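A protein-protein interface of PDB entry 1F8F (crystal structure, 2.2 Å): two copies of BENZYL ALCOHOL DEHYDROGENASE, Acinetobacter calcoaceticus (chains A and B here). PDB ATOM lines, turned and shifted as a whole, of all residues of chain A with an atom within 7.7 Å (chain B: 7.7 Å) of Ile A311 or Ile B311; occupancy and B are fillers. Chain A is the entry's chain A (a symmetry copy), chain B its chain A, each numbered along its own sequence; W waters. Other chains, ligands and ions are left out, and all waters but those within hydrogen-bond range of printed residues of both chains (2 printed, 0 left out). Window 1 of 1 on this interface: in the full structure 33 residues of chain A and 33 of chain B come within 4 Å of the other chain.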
ATOM      1  N   LEU A 272      29.908   1.358  12.710  1.00  0.00           N
ATOM      2  CA  LEU A 272      28.801   1.668  13.602  1.00  0.00           C
ATOM      3  C   LEU A 272      28.579   0.555  14.639  1.00  0.00           C
ATOM      4  O   LEU A 272      28.463   0.932  15.820  1.00  0.00           O
ATOM      5  CB  LEU A 272      27.553   1.940  12.783  1.00  0.00           C
ATOM      6  CG  LEU A 272      26.220   2.262  13.433  1.00  0.00           C
ATOM      7  CD1 LEU A 272      25.174   2.632  12.373  1.00  0.00           C
ATOM      8  CD2 LEU A 272      25.578   1.124  14.234  1.00  0.00           C
ATOM      9  N   GLY A 275      31.256   1.101  17.262  1.00  0.00           N
ATOM     10  CA  GLY A 275      30.832   2.200  18.096  1.00  0.00           C
ATOM     11  C   GLY A 275      29.852   1.798  19.207  1.00  0.00           C
ATOM     12  O   GLY A 275      30.086   2.256  20.328  1.00  0.00           O
ATOM     13  N   VAL A 276      28.878   0.946  18.975  1.00  0.00           N
ATOM     14  CA  VAL A 276      27.976   0.449  20.034  1.00  0.00           C
ATOM     15  C   VAL A 276      28.778  -0.459  20.933  1.00  0.00           C
ATOM     16  O   VAL A 276      28.748  -0.250  22.157  1.00  0.00           O
ATOM     17  CB  VAL A 276      26.746  -0.282  19.454  1.00  0.00           C
ATOM     18  CG1 VAL A 276      25.766  -0.689  20.543  1.00  0.00           C
ATOM     19  CG2 VAL A 276      25.998   0.611  18.495  1.00  0.00           C
ATOM     20  N   LEU A 279      30.983   1.444  23.801  1.00  0.00           N
ATOM     21  CA  LEU A 279      30.290   2.195  24.840  1.00  0.00           C
ATOM     22  C   LEU A 279      30.475   1.423  26.152  1.00  0.00           C
ATOM     23  O   LEU A 279      30.548   0.183  26.158  1.00  0.00           O
ATOM     24  CB  LEU A 279      28.835   2.268  24.447  1.00  0.00           C
ATOM     25  CG  LEU A 279      28.434   3.078  23.224  1.00  0.00           C
ATOM     26  CD1 LEU A 279      26.934   2.971  23.009  1.00  0.00           C
ATOM     27  CD2 LEU A 279      28.860   4.535  23.354  1.00  0.00           C
ATOM     28  N   GLY A 283      26.148   3.840  28.344  1.00  0.00           N
ATOM     29  CA  GLY A 283      26.640   4.727  27.288  1.00  0.00           C
ATOM     30  C   GLY A 283      25.627   5.028  26.208  1.00  0.00           C
ATOM     31  O   GLY A 283      24.610   4.321  26.016  1.00  0.00           O
ATOM     32  N   LYS A 284      25.877   6.099  25.448  1.00  0.00           N
ATOM     33  CA  LYS A 284      25.006   6.572  24.398  1.00  0.00           C
ATOM     34  C   LYS A 284      25.748   6.881  23.103  1.00  0.00           C
ATOM     35  O   LYS A 284      26.649   7.707  23.146  1.00  0.00           O
ATOM     36  CB  LYS A 284      24.185   7.806  24.838  1.00  0.00           C
ATOM     37  CG  LYS A 284      23.401   7.659  26.125  1.00  0.00           C
ATOM     38  CD  LYS A 284      22.535   8.894  26.430  1.00  0.00           C
ATOM     39  CE  LYS A 284      22.082   8.707  27.874  1.00  0.00           C
ATOM     40  NZ  LYS A 284      21.012   9.596  28.365  1.00  0.00           N
ATOM     41  N   ILE A 285      25.220   6.435  21.934  1.00  0.00           N
ATOM     42  CA  ILE A 285      25.904   6.750  20.690  1.00  0.00           C
ATOM     43  C   ILE A 285      24.935   7.449  19.748  1.00  0.00           C
ATOM     44  O   ILE A 285      23.835   6.933  19.501  1.00  0.00           O
ATOM     45  CB  ILE A 285      26.542   5.513  19.995  1.00  0.00           C
ATOM     46  CG1 ILE A 285      27.367   5.994  18.760  1.00  0.00           C
ATOM     47  CG2 ILE A 285      25.534   4.462  19.595  1.00  0.00           C
ATOM     48  CD1 ILE A 285      28.368   5.002  18.177  1.00  0.00           C
ATOM     49  N   ALA A 286      25.238   8.635  19.256  1.00  0.00           N
ATOM     50  CA  ALA A 286      24.413   9.394  18.342  1.00  0.00           C
ATOM     51  C   ALA A 286      24.789   9.089  16.878  1.00  0.00           C
ATOM     52  O   ALA A 286      25.969   9.217  16.578  1.00  0.00           O
ATOM     53  CB  ALA A 286      24.529  10.914  18.568  1.00  0.00           C
ATOM     54  N   VAL A 287      23.839   8.839  15.963  1.00  0.00           N
ATOM     55  CA  VAL A 287      24.133   8.505  14.600  1.00  0.00           C
ATOM     56  C   VAL A 287      23.930   9.648  13.626  1.00  0.00           C
ATOM     57  O   VAL A 287      22.777   9.978  13.395  1.00  0.00           O
ATOM     58  CB  VAL A 287      23.279   7.277  14.157  1.00  0.00           C
ATOM     59  CG1 VAL A 287      23.530   6.880  12.711  1.00  0.00           C
ATOM     60  CG2 VAL A 287      23.615   6.018  14.992  1.00  0.00           C
ATOM     61  N   ALA A 297      22.471  -1.774   9.584  1.00  0.00           N
ATOM     62  CA  ALA A 297      23.663  -2.059  10.399  1.00  0.00           C
ATOM     63  C   ALA A 297      23.249  -3.025  11.512  1.00  0.00           C
ATOM     64  O   ALA A 297      22.066  -3.157  11.825  1.00  0.00           O
ATOM     65  CB  ALA A 297      24.311  -0.812  10.973  1.00  0.00           C
ATOM     66  N   GLN A 298      24.196  -3.709  12.122  1.00  0.00           N
ATOM     67  CA  GLN A 298      24.008  -4.697  13.129  1.00  0.00           C
ATOM     68  C   GLN A 298      24.431  -4.278  14.517  1.00  0.00           C
ATOM     69  O   GLN A 298      25.364  -3.481  14.516  1.00  0.00           O
ATOM     70  CB  GLN A 298      24.995  -5.846  12.781  1.00  0.00           C
ATOM     71  CG  GLN A 298      24.345  -6.779  11.712  1.00  0.00           C
ATOM     72  CD  GLN A 298      25.406  -7.854  11.399  1.00  0.00           C
ATOM     73  OE1 GLN A 298      26.127  -7.763  10.402  1.00  0.00           O
ATOM     74  NE2 GLN A 298      25.595  -8.824  12.274  1.00  0.00           N
ATOM     75  N   PHE A 299      23.824  -4.801  15.566  1.00  0.00           N
ATOM     76  CA  PHE A 299      24.402  -4.574  16.908  1.00  0.00           C
ATOM     77  C   PHE A 299      24.253  -5.868  17.706  1.00  0.00           C
ATOM     78  O   PHE A 299      23.380  -6.671  17.399  1.00  0.00           O
ATOM     79  CB  PHE A 299      23.803  -3.340  17.516  1.00  0.00           C
ATOM     80  CG  PHE A 299      22.349  -3.444  17.827  1.00  0.00           C
ATOM     81  CD1 PHE A 299      21.306  -3.331  16.934  1.00  0.00           C
ATOM     82  CD2 PHE A 299      22.079  -3.694  19.163  1.00  0.00           C
ATOM     83  CE1 PHE A 299      19.992  -3.467  17.384  1.00  0.00           C
ATOM     84  CE2 PHE A 299      20.791  -3.847  19.622  1.00  0.00           C
ATOM     85  CZ  PHE A 299      19.763  -3.775  18.743  1.00  0.00           C
ATOM     86  N   ASP A 300      25.070  -6.182  18.671  1.00  0.00           N
ATOM     87  CA  ASP A 300      24.950  -7.338  19.552  1.00  0.00           C
ATOM     88  C   ASP A 300      23.809  -7.065  20.550  1.00  0.00           C
ATOM     89  O   ASP A 300      23.891  -6.117  21.337  1.00  0.00           O
ATOM     90  CB  ASP A 300      26.235  -7.574  20.306  1.00  0.00           C
ATOM     91  CG  ASP A 300      26.358  -8.721  21.256  1.00  0.00           C
ATOM     92  OD1 ASP A 300      25.576  -9.035  22.171  1.00  0.00           O
ATOM     93  OD2 ASP A 300      27.402  -9.428  21.126  1.00  0.00           O
ATOM     94  N   LEU A 304      23.842  -4.807  24.353  1.00  0.00           N
ATOM     95  CA  LEU A 304      23.083  -3.584  24.477  1.00  0.00           C
ATOM     96  C   LEU A 304      22.066  -3.672  25.604  1.00  0.00           C
ATOM     97  O   LEU A 304      21.790  -2.681  26.284  1.00  0.00           O
ATOM     98  CB  LEU A 304      22.396  -3.343  23.137  1.00  0.00           C
ATOM     99  CG  LEU A 304      21.347  -2.241  23.034  1.00  0.00           C
ATOM    100  CD1 LEU A 304      21.673  -1.272  21.896  1.00  0.00           C
ATOM    101  CD2 LEU A 304      19.940  -2.768  22.773  1.00  0.00           C
ATOM    102  N   GLY A 308      22.568  -1.504  29.233  1.00  0.00           N
ATOM    103  CA  GLY A 308      21.582  -0.418  29.217  1.00  0.00           C
ATOM    104  C   GLY A 308      21.893   0.706  28.215  1.00  0.00           C
ATOM    105  O   GLY A 308      21.675   1.921  28.422  1.00  0.00           O
ATOM    106  N   LYS A 309      22.496   0.252  27.124  1.00  0.00           N
ATOM    107  CA  LYS A 309      22.950   1.134  26.071  1.00  0.00           C
ATOM    108  C   LYS A 309      21.865   1.796  25.251  1.00  0.00           C
ATOM    109  O   LYS A 309      20.816   1.258  24.869  1.00  0.00           O
ATOM    110  CB  LYS A 309      23.929   0.304  25.197  1.00  0.00           C
ATOM    111  CG  LYS A 309      25.248  -0.032  25.895  1.00  0.00           C
ATOM    112  CD  LYS A 309      26.233  -0.762  24.926  1.00  0.00           C
ATOM    113  CE  LYS A 309      27.414  -1.199  25.783  1.00  0.00           C
ATOM    114  NZ  LYS A 309      28.426  -2.034  25.067  1.00  0.00           N
ATOM    115  N   THR A 310      22.126   3.021  24.815  1.00  0.00           N
ATOM    116  CA  THR A 310      21.254   3.773  23.930  1.00  0.00           C
ATOM    117  C   THR A 310      21.842   4.103  22.545  1.00  0.00           C
ATOM    118  O   THR A 310      22.968   4.557  22.325  1.00  0.00           O
ATOM    119  CB  THR A 310      20.732   5.066  24.557  1.00  0.00           C
ATOM    120  OG1 THR A 310      20.310   4.836  25.881  1.00  0.00           O
ATOM    121  CG2 THR A 310      19.571   5.539  23.698  1.00  0.00           C
ATOM    122  N   ILE A 311      21.036   3.820  21.536  1.00  0.00           N
ATOM    123  CA  ILE A 311      21.448   4.101  20.149  1.00  0.00           C
ATOM    124  C   ILE A 311      20.477   5.163  19.612  1.00  0.00           C
ATOM    125  O   ILE A 311      19.275   4.856  19.592  1.00  0.00           O
ATOM    126  CB  ILE A 311      21.414   2.863  19.259  1.00  0.00           C
ATOM    127  CG1 ILE A 311      22.462   1.751  19.394  1.00  0.00           C
ATOM    128  CG2 ILE A 311      21.651   3.256  17.816  1.00  0.00           C
ATOM    129  CD1 ILE A 311      21.963   0.529  18.568  1.00  0.00           C
ATOM    130  N   LEU A 312      20.879   6.362  19.194  1.00  0.00           N
ATOM    131  CA  LEU A 312      19.969   7.361  18.692  1.00  0.00           C
ATOM    132  C   LEU A 312      20.290   8.160  17.412  1.00  0.00           C
ATOM    133  O   LEU A 312      21.375   8.663  17.167  1.00  0.00           O
ATOM    134  CB  LEU A 312      19.581   8.470  19.695  1.00  0.00           C
ATOM    135  CG  LEU A 312      20.586   9.453  20.231  1.00  0.00           C
ATOM    136  CD1 LEU A 312      20.016  10.767  20.710  1.00  0.00           C
ATOM    137  CD2 LEU A 312      21.300   8.779  21.417  1.00  0.00           C
ATOM    138  N   GLY A 313      19.211   8.330  16.603  1.00  0.00           N
ATOM    139  CA  GLY A 313      19.343   9.042  15.339  1.00  0.00           C
ATOM    140  C   GLY A 313      19.343  10.552  15.419  1.00  0.00           C
ATOM    141  O   GLY A 313      18.410  11.051  16.090  1.00  0.00           O
ATOM    142  N   LEU B 272      12.572  -7.655  15.984  1.00  0.00           N
ATOM    143  CA  LEU B 272      13.158  -6.440  16.530  1.00  0.00           C
ATOM    144  C   LEU B 272      13.400  -5.386  15.437  1.00  0.00           C
ATOM    145  O   LEU B 272      12.994  -4.237  15.696  1.00  0.00           O
ATOM    146  CB  LEU B 272      14.431  -6.785  17.279  1.00  0.00           C
ATOM    147  CG  LEU B 272      15.290  -5.722  17.937  1.00  0.00           C
ATOM    148  CD1 LEU B 272      16.429  -6.364  18.741  1.00  0.00           C
ATOM    149  CD2 LEU B 272      15.988  -4.746  16.982  1.00  0.00           C
ATOM    150  N   GLY B 275      10.006  -3.832  14.794  1.00  0.00           N
ATOM    151  CA  GLY B 275       9.738  -2.908  15.870  1.00  0.00           C
ATOM    152  C   GLY B 275      10.384  -1.528  15.681  1.00  0.00           C
ATOM    153  O   GLY B 275       9.661  -0.556  15.910  1.00  0.00           O
ATOM    154  N   VAL B 276      11.609  -1.412  15.219  1.00  0.00           N
ATOM    155  CA  VAL B 276      12.235  -0.107  14.922  1.00  0.00           C
ATOM    156  C   VAL B 276      11.548   0.468  13.709  1.00  0.00           C
ATOM    157  O   VAL B 276      11.109   1.628  13.777  1.00  0.00           O
ATOM    158  CB  VAL B 276      13.758  -0.232  14.696  1.00  0.00           C
ATOM    159  CG1 VAL B 276      14.412   1.128  14.505  1.00  0.00           C
ATOM    160  CG2 VAL B 276      14.423  -0.881  15.884  1.00  0.00           C
ATOM    161  N   LEU B 279       8.029   2.407  14.466  1.00  0.00           N
ATOM    162  CA  LEU B 279       8.052   3.618  15.277  1.00  0.00           C
ATOM    163  C   LEU B 279       7.730   4.791  14.344  1.00  0.00           C
ATOM    164  O   LEU B 279       8.086   4.775  13.154  1.00  0.00           O
ATOM    165  CB  LEU B 279       9.439   3.743  15.858  1.00  0.00           C
ATOM    166  CG  LEU B 279       9.910   2.727  16.887  1.00  0.00           C
ATOM    167  CD1 LEU B 279      11.341   3.036  17.292  1.00  0.00           C
ATOM    168  CD2 LEU B 279       8.996   2.699  18.105  1.00  0.00           C
ATOM    169  N   GLY B 283      10.026   8.317  17.759  1.00  0.00           N
ATOM    170  CA  GLY B 283       9.629   7.154  18.554  1.00  0.00           C
ATOM    171  C   GLY B 283      10.767   6.482  19.285  1.00  0.00           C
ATOM    172  O   GLY B 283      11.969   6.650  18.969  1.00  0.00           O
ATOM    173  N   LYS B 284      10.427   5.678  20.297  1.00  0.00           N
ATOM    174  CA  LYS B 284      11.373   4.987  21.141  1.00  0.00           C
ATOM    175  C   LYS B 284      11.027   3.515  21.338  1.00  0.00           C
ATOM    176  O   LYS B 284       9.937   3.246  21.821  1.00  0.00           O
ATOM    177  CB  LYS B 284      11.536   5.676  22.514  1.00  0.00           C
ATOM    178  CG  LYS B 284      11.865   7.153  22.483  1.00  0.00           C
ATOM    179  CD  LYS B 284      12.112   7.730  23.888  1.00  0.00           C
ATOM    180  CE  LYS B 284      12.112   9.243  23.694  1.00  0.00           C
ATOM    181  NZ  LYS B 284      12.598  10.066  24.819  1.00  0.00           N
ATOM    182  N   ILE B 285      12.021   2.598  21.221  1.00  0.00           N
ATOM    183  CA  ILE B 285      11.710   1.193  21.438  1.00  0.00           C
ATOM    184  C   ILE B 285      12.631   0.635  22.513  1.00  0.00           C
ATOM    185  O   ILE B 285      13.858   0.780  22.409  1.00  0.00           O
ATOM    186  CB  ILE B 285      11.790   0.327  20.149  1.00  0.00           C
ATOM    187  CG1 ILE B 285      11.294  -1.117  20.476  1.00  0.00           C
ATOM    188  CG2 ILE B 285      13.167   0.298  19.530  1.00  0.00           C
ATOM    189  CD1 ILE B 285      10.935  -2.002  19.287  1.00  0.00           C
ATOM    190  N   ALA B 286      12.117   0.066  23.586  1.00  0.00           N
ATOM    191  CA  ALA B 286      12.881  -0.515  24.669  1.00  0.00           C
ATOM    192  C   ALA B 286      13.123  -2.019  24.426  1.00  0.00           C
ATOM    193  O   ALA B 286      12.133  -2.703  24.201  1.00  0.00           O
ATOM    194  CB  ALA B 286      12.188  -0.348  26.034  1.00  0.00           C
ATOM    195  N   VAL B 287      14.341  -2.555  24.600  1.00  0.00           N
ATOM    196  CA  VAL B 287      14.634  -3.935  24.345  1.00  0.00           C
ATOM    197  C   VAL B 287      14.737  -4.785  25.595  1.00  0.00           C
ATOM    198  O   VAL B 287      15.718  -4.612  26.302  1.00  0.00           O
ATOM    199  CB  VAL B 287      15.949  -4.056  23.515  1.00  0.00           C
ATOM    200  CG1 VAL B 287      16.327  -5.500  23.224  1.00  0.00           C
ATOM    201  CG2 VAL B 287      15.812  -3.382  22.128  1.00  0.00           C
ATOM    202  N   ALA B 297      21.215  -8.050  15.781  1.00  0.00           N
ATOM    203  CA  ALA B 297      19.996  -7.689  15.038  1.00  0.00           C
ATOM    204  C   ALA B 297      20.334  -6.498  14.137  1.00  0.00           C
ATOM    205  O   ALA B 297      21.323  -5.801  14.358  1.00  0.00           O
ATOM    206  CB  ALA B 297      18.815  -7.374  15.938  1.00  0.00           C
ATOM    207  N   GLN B 298      19.534  -6.244  13.121  1.00  0.00           N
ATOM    208  CA  GLN B 298      19.712  -5.231  12.138  1.00  0.00           C
ATOM    209  C   GLN B 298      18.750  -4.071  12.240  1.00  0.00           C
ATOM    210  O   GLN B 298      17.655  -4.393  12.690  1.00  0.00           O
ATOM    211  CB  GLN B 298      19.344  -5.890  10.781  1.00  0.00           C
ATOM    212  CG  GLN B 298      20.579  -6.670  10.233  1.00  0.00           C
ATOM    213  CD  GLN B 298      20.109  -7.322   8.917  1.00  0.00           C
ATOM    214  OE1 GLN B 298      19.760  -8.505   8.884  1.00  0.00           O
ATOM    215  NE2 GLN B 298      19.990  -6.561   7.846  1.00  0.00           N
ATOM    216  N   PHE B 299      19.128  -2.876  11.824  1.00  0.00           N
ATOM    217  CA  PHE B 299      18.108  -1.813  11.701  1.00  0.00           C
ATOM    218  C   PHE B 299      18.424  -1.006  10.443  1.00  0.00           C
ATOM    219  O   PHE B 299      19.568  -0.995  10.002  1.00  0.00           O
ATOM    220  CB  PHE B 299      18.022  -1.041  12.985  1.00  0.00           C
ATOM    221  CG  PHE B 299      19.243  -0.253  13.319  1.00  0.00           C
ATOM    222  CD1 PHE B 299      20.412  -0.738  13.861  1.00  0.00           C
ATOM    223  CD2 PHE B 299      19.137   1.096  13.020  1.00  0.00           C
ATOM    224  CE1 PHE B 299      21.475   0.134  14.105  1.00  0.00           C
ATOM    225  CE2 PHE B 299      20.180   1.967  13.238  1.00  0.00           C
ATOM    226  CZ  PHE B 299      21.346   1.490  13.736  1.00  0.00           C
ATOM    227  N   ASP B 300      17.500  -0.377   9.775  1.00  0.00           N
ATOM    228  CA  ASP B 300      17.716   0.496   8.628  1.00  0.00           C
ATOM    229  C   ASP B 300      18.311   1.822   9.138  1.00  0.00           C
ATOM    230  O   ASP B 300      17.663   2.531   9.914  1.00  0.00           O
ATOM    231  CB  ASP B 300      16.419   0.768   7.907  1.00  0.00           C
ATOM    232  CG  ASP B 300      16.395   1.624   6.683  1.00  0.00           C
ATOM    233  OD1 ASP B 300      16.899   2.752   6.535  1.00  0.00           O
ATOM    234  OD2 ASP B 300      15.756   1.149   5.697  1.00  0.00           O
ATOM    235  N   LEU B 304      16.291   5.380  10.821  1.00  0.00           N
ATOM    236  CA  LEU B 304      16.505   5.750  12.201  1.00  0.00           C
ATOM    237  C   LEU B 304      17.071   7.156  12.317  1.00  0.00           C
ATOM    238  O   LEU B 304      16.759   7.887  13.261  1.00  0.00           O
ATOM    239  CB  LEU B 304      17.460   4.724  12.800  1.00  0.00           C
ATOM    240  CG  LEU B 304      18.045   4.980  14.184  1.00  0.00           C
ATOM    241  CD1 LEU B 304      17.792   3.796  15.119  1.00  0.00           C
ATOM    242  CD2 LEU B 304      19.552   5.216  14.170  1.00  0.00           C
ATOM    243  N   GLY B 308      14.723  10.390  13.784  1.00  0.00           N
ATOM    244  CA  GLY B 308      15.230  10.707  15.124  1.00  0.00           C
ATOM    245  C   GLY B 308      14.894   9.655  16.194  1.00  0.00           C
ATOM    246  O   GLY B 308      14.606   9.920  17.383  1.00  0.00           O
ATOM    247  N   LYS B 309      14.867   8.426  15.697  1.00  0.00           N
ATOM    248  CA  LYS B 309      14.503   7.278  16.499  1.00  0.00           C
ATOM    249  C   LYS B 309      15.500   6.874  17.563  1.00  0.00           C
ATOM    250  O   LYS B 309      16.733   6.875  17.437  1.00  0.00           O
ATOM    251  CB  LYS B 309      14.202   6.126  15.503  1.00  0.00           C
ATOM    252  CG  LYS B 309      12.926   6.334  14.684  1.00  0.00           C
ATOM    253  CD  LYS B 309      12.616   5.090  13.791  1.00  0.00           C
ATOM    254  CE  LYS B 309      11.446   5.495  12.904  1.00  0.00           C
ATOM    255  NZ  LYS B 309      11.066   4.480  11.875  1.00  0.00           N
ATOM    256  N   THR B 310      14.993   6.371  18.680  1.00  0.00           N
ATOM    257  CA  THR B 310      15.791   5.834  19.767  1.00  0.00           C
ATOM    258  C   THR B 310      15.605   4.330  20.045  1.00  0.00           C
ATOM    259  O   THR B 310      14.526   3.739  20.135  1.00  0.00           O
ATOM    260  CB  THR B 310      15.611   6.597  21.080  1.00  0.00           C
ATOM    261  OG1 THR B 310      15.637   7.986  20.849  1.00  0.00           O
ATOM    262  CG2 THR B 310      16.751   6.182  21.994  1.00  0.00           C
ATOM    263  N   ILE B 311      16.737   3.657  20.152  1.00  0.00           N
ATOM    264  CA  ILE B 311      16.723   2.212  20.440  1.00  0.00           C
ATOM    265  C   ILE B 311      17.392   2.033  21.811  1.00  0.00           C
ATOM    266  O   ILE B 311      18.566   2.425  21.911  1.00  0.00           O
ATOM    267  CB  ILE B 311      17.461   1.391  19.388  1.00  0.00           C
ATOM    268  CG1 ILE B 311      16.869   1.165  17.990  1.00  0.00           C
ATOM    269  CG2 ILE B 311      17.581  -0.048  19.844  1.00  0.00           C
ATOM    270  CD1 ILE B 311      17.992   0.562  17.095  1.00  0.00           C
ATOM    271  N   LEU B 312      16.763   1.500  22.857  1.00  0.00           N
ATOM    272  CA  LEU B 312      17.388   1.334  24.145  1.00  0.00           C
ATOM    273  C   LEU B 312      17.244   0.019  24.938  1.00  0.00           C
ATOM    274  O   LEU B 312      16.192  -0.583  25.090  1.00  0.00           O
ATOM    275  CB  LEU B 312      17.031   2.406  25.200  1.00  0.00           C
ATOM    276  CG  LEU B 312      15.636   2.564  25.740  1.00  0.00           C
ATOM    277  CD1 LEU B 312      15.538   3.204  27.105  1.00  0.00           C
ATOM    278  CD2 LEU B 312      14.854   3.438  24.743  1.00  0.00           C
ATOM    279  N   GLY B 313      18.399  -0.375  25.535  1.00  0.00           N
ATOM    280  CA  GLY B 313      18.446  -1.611  26.305  1.00  0.00           C
ATOM    281  C   GLY B 313      17.905  -1.541  27.717  1.00  0.00           C
ATOM    282  O   GLY B 313      18.345  -0.594  28.410  1.00  0.00           O
HETATM  283  O   HOH W   1      18.660   2.028  29.317  1.00  0.00           O
HETATM  284  O   HOH W   2      16.947  11.788  18.352  1.00  0.00           O
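The backbone carbonyl oxygen of Lys B309 lies within hydrogen-bond range of the backbone NH of Gly A313. N of Phe B299 is in hydrogen-bond range of O of Ala A297 (3.0 Å). O of Ala B297 lies within hydrogen-bond range of N of Phe A299. The backbone carbonyl oxygen (O) of Ile A311 lies within hydrogen-bond range of the backbone NH (N) of Ile B311 (2.9 Å). O of Lys A309 is in hydrogen-bond range of N of Gly B313, 3.0 Å away.
The backbone NH (N) of Thr A310 lies within hydrogen-bond range of the backbone carbonyl oxygen (O) of Gly A283 (3.1 Å). The backbone carbonyl oxygen of Leu B304 is in hydrogen-bond range of the backbone NH of Lys B309 (3.1 Å). O of Leu B279 is in hydrogen-bond range of NZ of Lys B309 (3.3 Å). N of Thr B310 lies within hydrogen-bond range of O of Gly B283, 3.1 Å away. N of Val B287 is in hydrogen-bond range of O of Leu B312 (2.7 Å). N of Val A287 is in hydrogen-bond range of O of Leu A312 (2.7 Å).
Ala A297 touches Ala B297. O of Ala A297 touches CA of Gln B298, at 3.2 Å. Gly B313 touches Leu A304 (CA to O, 3.5 Å). Gly A308 touches Gly B313 (CA to O, 3.3 Å). O of Lys A309 touches O of Ile B311, at 3.9 Å. Leu B312 touches Lys A309 (CA to O, 3.5 Å). Thr A310 touches Thr B310 (CG2 to CG2, 3.4 Å). Ile A311 touches Lys B309. CA of Thr B310 touches O of Ile A311, at 3.6 Å. Leu A312 touches Lys B309.
Of the printed residues of chain B, Gly A308 touches Gly B313. Of the printed residues of chain B, Lys A309 touches Ile B311, Leu B312 and Gly B313. Ile A311 touches just these residues of chain B: Lys B309 (3.9 Å), Thr B310 (3.6 Å) and Ile B311 (2.9 Å). Of the printed residues of chain B, Gly A313 touches Leu B304 (3.5 Å), Gly B308 (3.3 Å) and Lys B309 (3.0 Å). Lys B284 touches none of the printed residues of chain A. Val B287 touches none of the printed residues of chain A. Of the printed residues of chain A, Ala B297 touches Ala A297 (3.7 Å), Gln A298 (3.2 Å) and Phe A299 (3.0 Å). Of chain A, only Lys A309, Thr A310 and Ile A311 come within 4 Å of Ile B311. Of the printed residues of chain A, Leu B312 touches Lys A309.
Along chain A the printed residues that touch a printed residue of chain B span positions 297 to 313. Among the printed residues, 19 pairs touch across the chains. Among the printed residues, no Asp or Glu carboxylate lies within 4 Å of a Lys or Arg side-chain nitrogen of the other chain.
Ala A297 touches Phe B299, and with the chains exchanged Phe A299 touches Ala B297. Lys A309 touches Ile B311, and with the chains exchanged Ile A311 touches Lys B309. Lys A309 touches Gly B313, and with the chains exchanged Gly A313 touches Lys B309. Ile B311 touches its own counterpart, Ile A311. Of the 19 pairs that touch across the chains among the printed residues, 19 have their exchanged pair printed and touching as well.
Water W1 bridges the backbone carbonyl oxygen (O) of Gly B313 (2.8 Å) and the backbone carbonyl oxygen (O) of Gly A308 (3.1 Å). Water W2 bridges O of Gly A313 (2.8 Å) and O of Gly B308 (3.1 Å).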
